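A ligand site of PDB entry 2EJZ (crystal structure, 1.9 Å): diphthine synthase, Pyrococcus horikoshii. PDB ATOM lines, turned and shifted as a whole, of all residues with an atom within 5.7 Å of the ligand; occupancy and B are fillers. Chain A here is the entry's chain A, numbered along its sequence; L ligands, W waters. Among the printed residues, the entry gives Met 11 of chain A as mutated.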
ATOM      1  N   LEU A  10      -7.247 -20.365 -23.103  1.00  0.00           N
ATOM      2  CA  LEU A  10      -8.407 -20.615 -22.247  1.00  0.00           C
ATOM      3  C   LEU A  10      -9.769 -20.999 -22.801  1.00  0.00           C
ATOM      4  O   LEU A  10     -10.350 -21.993 -22.375  1.00  0.00           O
ATOM      5  CB  LEU A  10      -8.620 -19.396 -21.356  1.00  0.00           C
ATOM      6  CG  LEU A  10      -7.560 -19.064 -20.314  1.00  0.00           C
ATOM      7  CD1 LEU A  10      -7.735 -17.626 -19.836  1.00  0.00           C
ATOM      8  CD2 LEU A  10      -7.677 -20.034 -19.161  1.00  0.00           C
ATOM      9  N   MET A  11     -10.286 -20.203 -23.732  1.00  0.00           N
ATOM     10  CA  MET A  11     -11.633 -20.432 -24.229  1.00  0.00           C
ATOM     11  C   MET A  11     -11.855 -20.697 -25.706  1.00  0.00           C
ATOM     12  O   MET A  11     -12.595 -21.613 -26.060  1.00  0.00           O
ATOM     13  CB  MET A  11     -12.496 -19.241 -23.823  1.00  0.00           C
ATOM     14  CG  MET A  11     -13.980 -19.451 -24.032  1.00  0.00           C
ATOM     15  SD  MET A  11     -14.678 -20.323 -22.638  1.00  0.00           S
ATOM     16  CE  MET A  11     -14.217 -22.040 -22.987  1.00  0.00           C
ATOM     17  N   THR A  36      -7.740 -32.666 -22.798  1.00  0.00           N
ATOM     18  CA  THR A  36      -7.196 -32.182 -21.525  1.00  0.00           C
ATOM     19  C   THR A  36      -7.999 -31.034 -20.937  1.00  0.00           C
ATOM     20  O   THR A  36      -7.855 -30.700 -19.764  1.00  0.00           O
ATOM     21  CB  THR A  36      -5.711 -31.755 -21.653  1.00  0.00           C
ATOM     22  OG1 THR A  36      -5.568 -30.783 -22.706  1.00  0.00           O
ATOM     23  CG2 THR A  36      -4.832 -32.955 -21.939  1.00  0.00           C
ATOM     24  N   SER A  37      -8.859 -30.422 -21.756  1.00  0.00           N
ATOM     25  CA  SER A  37      -9.708 -29.335 -21.295  1.00  0.00           C
ATOM     26  C   SER A  37     -10.816 -29.096 -22.305  1.00  0.00           C
ATOM     27  O   SER A  37     -10.841 -29.730 -23.355  1.00  0.00           O
ATOM     28  CB  SER A  37      -8.891 -28.045 -21.093  1.00  0.00           C
ATOM     29  OG  SER A  37      -9.683 -27.055 -20.453  1.00  0.00           O
ATOM     30  N   LEU A  38     -11.716 -28.175 -21.980  1.00  0.00           N
ATOM     31  CA  LEU A  38     -12.831 -27.866 -22.868  1.00  0.00           C
ATOM     32  C   LEU A  38     -12.751 -26.444 -23.405  1.00  0.00           C
ATOM     33  O   LEU A  38     -12.675 -25.487 -22.633  1.00  0.00           O
ATOM     34  CB  LEU A  38     -14.165 -28.052 -22.133  1.00  0.00           C
ATOM     35  CG  LEU A  38     -15.444 -27.655 -22.875  1.00  0.00           C
ATOM     36  CD1 LEU A  38     -15.609 -28.521 -24.123  1.00  0.00           C
ATOM     37  CD2 LEU A  38     -16.639 -27.803 -21.955  1.00  0.00           C
ATOM     38  N   PRO A  85      -5.394 -27.230 -25.574  1.00  0.00           N
ATOM     39  CA  PRO A  85      -6.158 -26.174 -24.906  1.00  0.00           C
ATOM     40  C   PRO A  85      -5.230 -25.509 -23.871  1.00  0.00           C
ATOM     41  O   PRO A  85      -4.276 -26.142 -23.424  1.00  0.00           O
ATOM     42  CB  PRO A  85      -7.299 -26.934 -24.239  1.00  0.00           C
ATOM     43  CG  PRO A  85      -7.489 -28.124 -25.145  1.00  0.00           C
ATOM     44  CD  PRO A  85      -6.073 -28.534 -25.468  1.00  0.00           C
ATOM     45  N   GLY A  86      -5.532 -24.273 -23.497  1.00  0.00           N
ATOM     46  CA  GLY A  86      -4.726 -23.558 -22.510  1.00  0.00           C
ATOM     47  C   GLY A  86      -3.233 -23.597 -22.789  1.00  0.00           C
ATOM     48  O   GLY A  86      -2.813 -23.406 -23.929  1.00  0.00           O
ATOM     49  N   ASP A  87      -2.426 -23.818 -21.755  1.00  0.00           N
ATOM     50  CA  ASP A  87      -0.977 -23.933 -21.925  1.00  0.00           C
ATOM     51  C   ASP A  87      -0.749 -25.445 -22.002  1.00  0.00           C
ATOM     52  O   ASP A  87      -1.260 -26.201 -21.172  1.00  0.00           O
ATOM     53  CB  ASP A  87      -0.245 -23.323 -20.734  1.00  0.00           C
ATOM     54  CG  ASP A  87       1.263 -23.437 -20.859  1.00  0.00           C
ATOM     55  OD1 ASP A  87       1.786 -24.568 -20.834  1.00  0.00           O
ATOM     56  OD2 ASP A  87       1.936 -22.382 -20.983  1.00  0.00           O
ATOM     57  N   PRO A  88       0.045 -25.916 -22.987  1.00  0.00           N
ATOM     58  CA  PRO A  88       0.343 -27.345 -23.187  1.00  0.00           C
ATOM     59  C   PRO A  88       0.883 -28.148 -22.021  1.00  0.00           C
ATOM     60  O   PRO A  88       0.599 -29.342 -21.904  1.00  0.00           O
ATOM     61  CB  PRO A  88       1.334 -27.336 -24.354  1.00  0.00           C
ATOM     62  CG  PRO A  88       1.353 -25.967 -24.986  1.00  0.00           C
ATOM     63  CD  PRO A  88       0.859 -25.077 -23.892  1.00  0.00           C
ATOM     64  N   LEU A  89       1.661 -27.514 -21.153  1.00  0.00           N
ATOM     65  CA  LEU A  89       2.302 -28.211 -20.047  1.00  0.00           C
ATOM     66  C   LEU A  89       1.681 -28.062 -18.662  1.00  0.00           C
ATOM     67  O   LEU A  89       2.173 -28.642 -17.700  1.00  0.00           O
ATOM     68  CB  LEU A  89       3.771 -27.772 -19.978  1.00  0.00           C
ATOM     69  CG  LEU A  89       4.489 -27.694 -21.333  1.00  0.00           C
ATOM     70  CD1 LEU A  89       5.937 -27.290 -21.126  1.00  0.00           C
ATOM     71  CD2 LEU A  89       4.392 -29.034 -22.052  1.00  0.00           C
ATOM     72  N   VAL A  90       0.606 -27.292 -18.551  1.00  0.00           N
ATOM     73  CA  VAL A  90      -0.043 -27.070 -17.271  1.00  0.00           C
ATOM     74  C   VAL A  90      -1.153 -28.075 -16.979  1.00  0.00           C
ATOM     75  O   VAL A  90      -2.159 -28.143 -17.692  1.00  0.00           O
ATOM     76  CB  VAL A  90      -0.640 -25.635 -17.205  1.00  0.00           C
ATOM     77  CG1 VAL A  90      -1.427 -25.453 -15.913  1.00  0.00           C
ATOM     78  CG2 VAL A  90       0.482 -24.613 -17.305  1.00  0.00           C
ATOM     79  N   ALA A  91      -0.962 -28.847 -15.920  1.00  0.00           N
ATOM     80  CA  ALA A  91      -1.949 -29.853 -15.507  1.00  0.00           C
ATOM     81  C   ALA A  91      -2.211 -30.890 -16.592  1.00  0.00           C
ATOM     82  O   ALA A  91      -3.347 -31.335 -16.780  1.00  0.00           O
ATOM     83  CB  ALA A  91      -3.264 -29.164 -15.103  1.00  0.00           C
ATOM     84  N   THR A  92      -1.151 -31.262 -17.297  1.00  0.00           N
ATOM     85  CA  THR A  92      -1.146 -32.319 -18.282  1.00  0.00           C
ATOM     86  C   THR A  92       0.127 -33.124 -18.122  1.00  0.00           C
ATOM     87  O   THR A  92       1.018 -32.784 -17.361  1.00  0.00           O
ATOM     88  CB  THR A  92      -1.170 -31.717 -19.707  1.00  0.00           C
ATOM     89  OG1 THR A  92       0.115 -31.166 -20.021  1.00  0.00           O
ATOM     90  CG2 THR A  92      -2.238 -30.621 -19.839  1.00  0.00           C
ATOM     91  N   PRO A 114      -2.565 -18.425 -22.658  1.00  0.00           N
ATOM     92  CA  PRO A 114      -3.230 -18.175 -21.370  1.00  0.00           C
ATOM     93  C   PRO A 114      -3.649 -19.507 -20.737  1.00  0.00           C
ATOM     94  O   PRO A 114      -4.167 -20.383 -21.427  1.00  0.00           O
ATOM     95  CB  PRO A 114      -4.452 -17.340 -21.747  1.00  0.00           C
ATOM     96  CG  PRO A 114      -4.056 -16.693 -23.028  1.00  0.00           C
ATOM     97  CD  PRO A 114      -3.282 -17.742 -23.753  1.00  0.00           C
ATOM     98  N   SER A 115      -3.426 -19.635 -19.440  1.00  0.00           N
ATOM     99  CA  SER A 115      -3.737 -20.861 -18.706  1.00  0.00           C
ATOM    100  C   SER A 115      -4.712 -20.602 -17.570  1.00  0.00           C
ATOM    101  O   SER A 115      -4.715 -19.524 -16.993  1.00  0.00           O
ATOM    102  CB  SER A 115      -2.447 -21.450 -18.129  1.00  0.00           C
ATOM    103  OG  SER A 115      -2.716 -22.548 -17.288  1.00  0.00           O
ATOM    104  N   ILE A 116      -5.551 -21.587 -17.240  1.00  0.00           N
ATOM    105  CA  ILE A 116      -6.484 -21.373 -16.139  1.00  0.00           C
ATOM    106  C   ILE A 116      -5.697 -21.166 -14.843  1.00  0.00           C
ATOM    107  O   ILE A 116      -6.170 -20.503 -13.924  1.00  0.00           O
ATOM    108  CB  ILE A 116      -7.447 -22.593 -15.954  1.00  0.00           C
ATOM    109  CG1 ILE A 116      -8.510 -22.266 -14.900  1.00  0.00           C
ATOM    110  CG2 ILE A 116      -6.648 -23.821 -15.513  1.00  0.00           C
ATOM    111  CD1 ILE A 116      -9.455 -21.140 -15.291  1.00  0.00           C
ATOM    112  N   TYR A 117      -4.489 -21.719 -14.775  1.00  0.00           N
ATOM    113  CA  TYR A 117      -3.668 -21.588 -13.575  1.00  0.00           C
ATOM    114  C   TYR A 117      -3.345 -20.146 -13.216  1.00  0.00           C
ATOM    115  O   TYR A 117      -3.272 -19.789 -12.026  1.00  0.00           O
ATOM    116  CB  TYR A 117      -2.381 -22.395 -13.734  1.00  0.00           C
ATOM    117  CG  TYR A 117      -1.600 -22.540 -12.442  1.00  0.00           C
ATOM    118  CD1 TYR A 117      -2.067 -23.345 -11.405  1.00  0.00           C
ATOM    119  CD2 TYR A 117      -0.388 -21.865 -12.263  1.00  0.00           C
ATOM    120  CE1 TYR A 117      -1.356 -23.487 -10.222  1.00  0.00           C
ATOM    121  CE2 TYR A 117       0.336 -21.993 -11.076  1.00  0.00           C
ATOM    122  CZ  TYR A 117      -0.151 -22.797 -10.069  1.00  0.00           C
ATOM    123  OH  TYR A 117       0.562 -22.936  -8.908  1.00  0.00           O
ATOM    124  N   LEU A 164      -8.757 -25.925  -7.390  1.00  0.00           N
ATOM    125  CA  LEU A 164      -9.200 -27.282  -7.685  1.00  0.00           C
ATOM    126  C   LEU A 164      -9.598 -27.434  -9.150  1.00  0.00           C
ATOM    127  O   LEU A 164     -10.633 -26.931  -9.568  1.00  0.00           O
ATOM    128  CB  LEU A 164     -10.396 -27.634  -6.806  1.00  0.00           C
ATOM    129  CG  LEU A 164     -10.158 -27.655  -5.291  1.00  0.00           C
ATOM    130  CD1 LEU A 164     -11.496 -27.666  -4.553  1.00  0.00           C
ATOM    131  CD2 LEU A 164      -9.323 -28.880  -4.928  1.00  0.00           C
ATOM    132  N   PHE A 165      -8.752 -28.106  -9.932  1.00  0.00           N
ATOM    133  CA  PHE A 165      -9.060 -28.368 -11.327  1.00  0.00           C
ATOM    134  C   PHE A 165     -10.217 -29.366 -11.241  1.00  0.00           C
ATOM    135  O   PHE A 165     -10.264 -30.151 -10.307  1.00  0.00           O
ATOM    136  CB  PHE A 165      -7.894 -29.040 -12.059  1.00  0.00           C
ATOM    137  CG  PHE A 165      -6.668 -28.188 -12.171  1.00  0.00           C
ATOM    138  CD1 PHE A 165      -6.517 -27.296 -13.224  1.00  0.00           C
ATOM    139  CD2 PHE A 165      -5.638 -28.286 -11.229  1.00  0.00           C
ATOM    140  CE1 PHE A 165      -5.368 -26.509 -13.353  1.00  0.00           C
ATOM    141  CE2 PHE A 165      -4.487 -27.503 -11.349  1.00  0.00           C
ATOM    142  CZ  PHE A 165      -4.347 -26.609 -12.421  1.00  0.00           C
ATOM    143  N   LEU A 166     -11.142 -29.326 -12.195  1.00  0.00           N
ATOM    144  CA  LEU A 166     -12.262 -30.259 -12.152  1.00  0.00           C
ATOM    145  C   LEU A 166     -12.086 -31.315 -13.225  1.00  0.00           C
ATOM    146  O   LEU A 166     -11.491 -31.064 -14.281  1.00  0.00           O
ATOM    147  CB  LEU A 166     -13.586 -29.495 -12.299  1.00  0.00           C
ATOM    148  CG  LEU A 166     -13.781 -28.406 -11.227  1.00  0.00           C
ATOM    149  CD1 LEU A 166     -15.230 -27.898 -11.261  1.00  0.00           C
ATOM    150  CD2 LEU A 166     -13.483 -28.982  -9.831  1.00  0.00           C
ATOM    151  N   ASP A 167     -12.596 -32.517 -12.965  1.00  0.00           N
ATOM    152  CA  ASP A 167     -12.425 -33.624 -13.901  1.00  0.00           C
ATOM    153  C   ASP A 167     -13.081 -33.436 -15.270  1.00  0.00           C
ATOM    154  O   ASP A 167     -14.009 -32.636 -15.447  1.00  0.00           O
ATOM    155  CB  ASP A 167     -12.929 -34.927 -13.278  1.00  0.00           C
ATOM    156  CG  ASP A 167     -12.107 -36.139 -13.720  1.00  0.00           C
ATOM    157  OD1 ASP A 167     -11.296 -36.019 -14.666  1.00  0.00           O
ATOM    158  OD2 ASP A 167     -12.284 -37.215 -13.111  1.00  0.00           O
ATOM    159  N   ILE A 168     -12.577 -34.187 -16.233  1.00  0.00           N
ATOM    160  CA  ILE A 168     -13.071 -34.147 -17.594  1.00  0.00           C
ATOM    161  C   ILE A 168     -12.852 -35.500 -18.257  1.00  0.00           C
ATOM    162  O   ILE A 168     -11.765 -36.088 -18.155  1.00  0.00           O
ATOM    163  CB  ILE A 168     -12.350 -33.054 -18.419  1.00  0.00           C
ATOM    164  CG1 ILE A 168     -12.725 -33.181 -19.900  1.00  0.00           C
ATOM    165  CG2 ILE A 168     -10.836 -33.157 -18.226  1.00  0.00           C
ATOM    166  CD1 ILE A 168     -12.078 -32.123 -20.795  1.00  0.00           C
ATOM    167  N   LEU A 206     -15.123 -20.069 -10.895  1.00  0.00           N
ATOM    168  CA  LEU A 206     -14.742 -19.333 -12.089  1.00  0.00           C
ATOM    169  C   LEU A 206     -15.139 -20.230 -13.239  1.00  0.00           C
ATOM    170  O   LEU A 206     -14.633 -21.351 -13.379  1.00  0.00           O
ATOM    171  CB  LEU A 206     -13.226 -19.072 -12.105  1.00  0.00           C
ATOM    172  CG  LEU A 206     -12.654 -18.430 -13.373  1.00  0.00           C
ATOM    173  CD1 LEU A 206     -13.372 -17.121 -13.684  1.00  0.00           C
ATOM    174  CD2 LEU A 206     -11.161 -18.184 -13.171  1.00  0.00           C
ATOM    175  N   ALA A 207     -16.060 -19.743 -14.066  1.00  0.00           N
ATOM    176  CA  ALA A 207     -16.533 -20.526 -15.205  1.00  0.00           C
ATOM    177  C   ALA A 207     -16.280 -19.813 -16.519  1.00  0.00           C
ATOM    178  O   ALA A 207     -16.542 -18.620 -16.655  1.00  0.00           O
ATOM    179  CB  ALA A 207     -18.036 -20.812 -15.054  1.00  0.00           C
ATOM    180  N   ARG A 208     -15.747 -20.566 -17.479  1.00  0.00           N
ATOM    181  CA  ARG A 208     -15.452 -20.065 -18.803  1.00  0.00           C
ATOM    182  C   ARG A 208     -14.489 -18.872 -18.806  1.00  0.00           C
ATOM    183  O   ARG A 208     -14.736 -17.850 -19.469  1.00  0.00           O
ATOM    184  CB  ARG A 208     -16.759 -19.716 -19.530  1.00  0.00           C
ATOM    185  CG  ARG A 208     -17.732 -20.911 -19.584  1.00  0.00           C
ATOM    186  CD  ARG A 208     -19.044 -20.524 -20.277  1.00  0.00           C
ATOM    187  NE  ARG A 208     -19.634 -19.339 -19.651  1.00  0.00           N
ATOM    188  CZ  ARG A 208     -20.195 -19.325 -18.447  1.00  0.00           C
ATOM    189  NH1 ARG A 208     -20.267 -20.427 -17.715  1.00  0.00           N
ATOM    190  NH2 ARG A 208     -20.661 -18.179 -17.953  1.00  0.00           N
ATOM    191  N   ALA A 209     -13.411 -19.002 -18.055  1.00  0.00           N
ATOM    192  CA  ALA A 209     -12.395 -17.961 -18.014  1.00  0.00           C
ATOM    193  C   ALA A 209     -11.941 -17.810 -19.463  1.00  0.00           C
ATOM    194  O   ALA A 209     -11.993 -18.763 -20.226  1.00  0.00           O
ATOM    195  CB  ALA A 209     -11.223 -18.398 -17.127  1.00  0.00           C
ATOM    196  N   GLY A 210     -11.502 -16.618 -19.839  1.00  0.00           N
ATOM    197  CA  GLY A 210     -11.075 -16.421 -21.210  1.00  0.00           C
ATOM    198  C   GLY A 210     -12.191 -15.821 -22.056  1.00  0.00           C
ATOM    199  O   GLY A 210     -11.940 -15.088 -23.010  1.00  0.00           O
ATOM    200  N   PRO A 233     -16.183 -25.047 -19.165  1.00  0.00           N
ATOM    201  CA  PRO A 233     -15.446 -25.552 -18.012  1.00  0.00           C
ATOM    202  C   PRO A 233     -15.526 -24.687 -16.764  1.00  0.00           C
ATOM    203  O   PRO A 233     -15.723 -23.475 -16.847  1.00  0.00           O
ATOM    204  CB  PRO A 233     -14.024 -25.656 -18.554  1.00  0.00           C
ATOM    205  CG  PRO A 233     -13.944 -24.450 -19.418  1.00  0.00           C
ATOM    206  CD  PRO A 233     -15.273 -24.463 -20.162  1.00  0.00           C
ATOM    207  N   HIS A 234     -15.382 -25.326 -15.610  1.00  0.00           N
ATOM    208  CA  HIS A 234     -15.425 -24.657 -14.314  1.00  0.00           C
ATOM    209  C   HIS A 234     -14.215 -25.071 -13.483  1.00  0.00           C
ATOM    210  O   HIS A 234     -13.635 -26.126 -13.699  1.00  0.00           O
ATOM    211  CB  HIS A 234     -16.630 -25.106 -13.463  1.00  0.00           C
ATOM    212  CG  HIS A 234     -17.972 -24.769 -14.037  1.00  0.00           C
ATOM    213  ND1 HIS A 234     -19.140 -25.095 -13.383  1.00  0.00           N
ATOM    214  CD2 HIS A 234     -18.344 -24.141 -15.176  1.00  0.00           C
ATOM    215  CE1 HIS A 234     -20.176 -24.687 -14.097  1.00  0.00           C
ATOM    216  NE2 HIS A 234     -19.716 -24.105 -15.184  1.00  0.00           N
ATOM    217  N   ILE A 235     -13.851 -24.211 -12.532  1.00  0.00           N
ATOM    218  CA  ILE A 235     -12.811 -24.544 -11.557  1.00  0.00           C
ATOM    219  C   ILE A 235     -13.441 -24.118 -10.251  1.00  0.00           C
ATOM    220  O   ILE A 235     -14.306 -23.225 -10.229  1.00  0.00           O
ATOM    221  CB  ILE A 235     -11.454 -23.779 -11.714  1.00  0.00           C
ATOM    222  CG1 ILE A 235     -11.665 -22.266 -11.699  1.00  0.00           C
ATOM    223  CG2 ILE A 235     -10.740 -24.257 -12.940  1.00  0.00           C
ATOM    224  CD1 ILE A 235     -10.418 -21.497 -11.233  1.00  0.00           C
HETATM  225  N1  LIG L   1      -3.427 -26.961 -19.721  1.00  0.00           N
HETATM  226  C1  LIG L   1      -4.758 -26.387 -19.270  1.00  0.00           C
HETATM  227  C2  LIG L   1      -5.424 -27.050 -18.096  1.00  0.00           C
HETATM  228  C3  LIG L   1      -5.742 -28.551 -18.185  1.00  0.00           C
HETATM  229  S1  LIG L   1      -6.783 -29.016 -16.730  1.00  0.00           S
HETATM  230  C4  LIG L   1      -4.510 -24.845 -18.991  1.00  0.00           C
HETATM  231  O1  LIG L   1      -3.360 -24.382 -19.145  1.00  0.00           O
HETATM  232  O2  LIG L   1      -5.527 -24.156 -18.612  1.00  0.00           O
HETATM  233  C5  LIG L   1      -8.381 -28.732 -17.386  1.00  0.00           C
HETATM  234  C6  LIG L   1      -9.351 -28.237 -16.240  1.00  0.00           C
HETATM  235  O3  LIG L   1      -8.927 -26.898 -15.869  1.00  0.00           O
HETATM  236  C7  LIG L   1     -10.788 -28.142 -16.608  1.00  0.00           C
HETATM  237  O4  LIG L   1     -11.446 -29.385 -16.392  1.00  0.00           O
HETATM  238  C8  LIG L   1     -11.253 -26.977 -15.708  1.00  0.00           C
HETATM  239  O5  LIG L   1     -11.555 -27.402 -14.376  1.00  0.00           O
HETATM  240  C9  LIG L   1     -10.095 -25.971 -15.779  1.00  0.00           C
HETATM  241  N2  LIG L   1     -10.136 -25.129 -16.847  1.00  0.00           N
HETATM  242  C10 LIG L   1      -9.465 -25.049 -18.061  1.00  0.00           C
HETATM  243  N3  LIG L   1      -9.813 -24.055 -18.821  1.00  0.00           N
HETATM  244  C11 LIG L   1     -10.812 -23.379 -18.081  1.00  0.00           C
HETATM  245  C12 LIG L   1     -11.587 -22.192 -18.375  1.00  0.00           C
HETATM  246  N4  LIG L   1     -11.483 -21.485 -19.517  1.00  0.00           N
HETATM  247  N5  LIG L   1     -12.472 -21.832 -17.393  1.00  0.00           N
HETATM  248  C13 LIG L   1     -12.631 -22.519 -16.227  1.00  0.00           C
HETATM  249  N6  LIG L   1     -11.909 -23.647 -15.910  1.00  0.00           N
HETATM  250  C14 LIG L   1     -11.021 -24.016 -16.875  1.00  0.00           C
HETATM  251  O   HOH W   1      -7.522 -24.355 -20.647  1.00  0.00           O
HETATM  252  O   HOH W   2      -4.428 -28.402 -21.800  1.00  0.00           O
HETATM  253  O   HOH W   3     -10.028 -24.843 -21.818  1.00  0.00           O
HETATM  254  O   HOH W   4     -14.045 -30.091 -17.020  1.00  0.00           O
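An oxygen (O1) of the ligand sits at hydrogen-bond distance from the backbone NH (N) of Asp 87 (2.8 Å). An oxygen (O4) of the ligand sits at hydrogen-bond distance from the backbone carbonyl oxygen of Leu 166 (2.7 Å). The backbone carbonyl oxygen of Ala 209 lies within hydrogen-bond range of a nitrogen (N4) of the ligand (2.9 Å). O of Asp 87 lies within hydrogen-bond range of N1 of the ligand (2.7 Å). The backbone NH (N) of Leu 166 lies within hydrogen-bond range of an oxygen (O5) of the ligand. N4 of the ligand sits at hydrogen-bond distance from O of Leu 10 (3.1 Å). The backbone NH of Ile 116 lies within hydrogen-bond range of an oxygen (O2) of the ligand, 2.9 Å away. The side-chain hydroxyl of Ser 115 lies within hydrogen-bond range of an oxygen (O1) of the ligand, 2.7 Å away. N3 of the ligand lies close to OG of Ser 37, at 3.4 Å. A nitrogen (N5) of the ligand sits at hydrogen-bond distance from the backbone NH (N) of Ala 209 (3.1 Å). The backbone carbonyl oxygen (O) of His 234 lies within hydrogen-bond range of an oxygen (O5) of the ligand, at 2.5 Å. A nitrogen (N1) of the ligand is in hydrogen-bond range of the backbone carbonyl oxygen of Val 90 (2.7 Å).
OG1 of Thr 92 lies within hydrogen-bond range of O of Pro 88 (2.7 Å). The side-chain carboxylate (OD1) of Asp 87 lies within hydrogen-bond range of the backbone NH (N) of Leu 89, 3.0 Å away. O of Leu 206 sits at hydrogen-bond distance from N of Ile 235, at 3.1 Å. The side-chain hydroxyl of Ser 115 sits close to the backbone NH of Tyr 117. N of Arg 208 is in hydrogen-bond range of O of Pro 233, 3.0 Å away.
O of Thr 36 sits close to S1 of the ligand (3.6 Å). Pro 85 touches the ligand (O to N1, 3.9 Å). Gly 86 touches the ligand. CB of Ala 91 touches S1 of the ligand, 3.9 Å away. CG2 of Thr 92 touches N1 of the ligand (3.9 Å). Phe 165 touches the ligand. Leu 206 touches the ligand. Arg 208 touches the ligand. Pro 233 touches the ligand. Ile 235 touches the ligand (CG2 to N6, 3.2 Å). Within 4 Å of the ligand: Leu 10, Thr 36, Ser 37, Pro 85, Gly 86, Asp 87, Val 90, Ala 91, Thr 92, Ser 115, Ile 116, Phe 165, Leu 166, Leu 206, Arg 208, Ala 209, Pro 233, His 234 and Ile 235. The nearest printed residue that does not touch the ligand is Ile 168 (4.2 Å).
Water W2 lies within hydrogen-bond range of a nitrogen (N1) of the ligand (2.7 Å), the backbone carbonyl oxygen (O) of Pro 85 (2.8 Å) and the side-chain hydroxyl (OG1) of Thr 36 (2.8 Å). Water W4 bridges O4 of the ligand (2.8 Å) and O of Asp 167 (3.0 Å). Water W1 lies within hydrogen-bond range of O2 of the ligand (2.9 Å), OG of Ser 37 (3.5 Å) and N of Gly 86 (3.5 Å).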
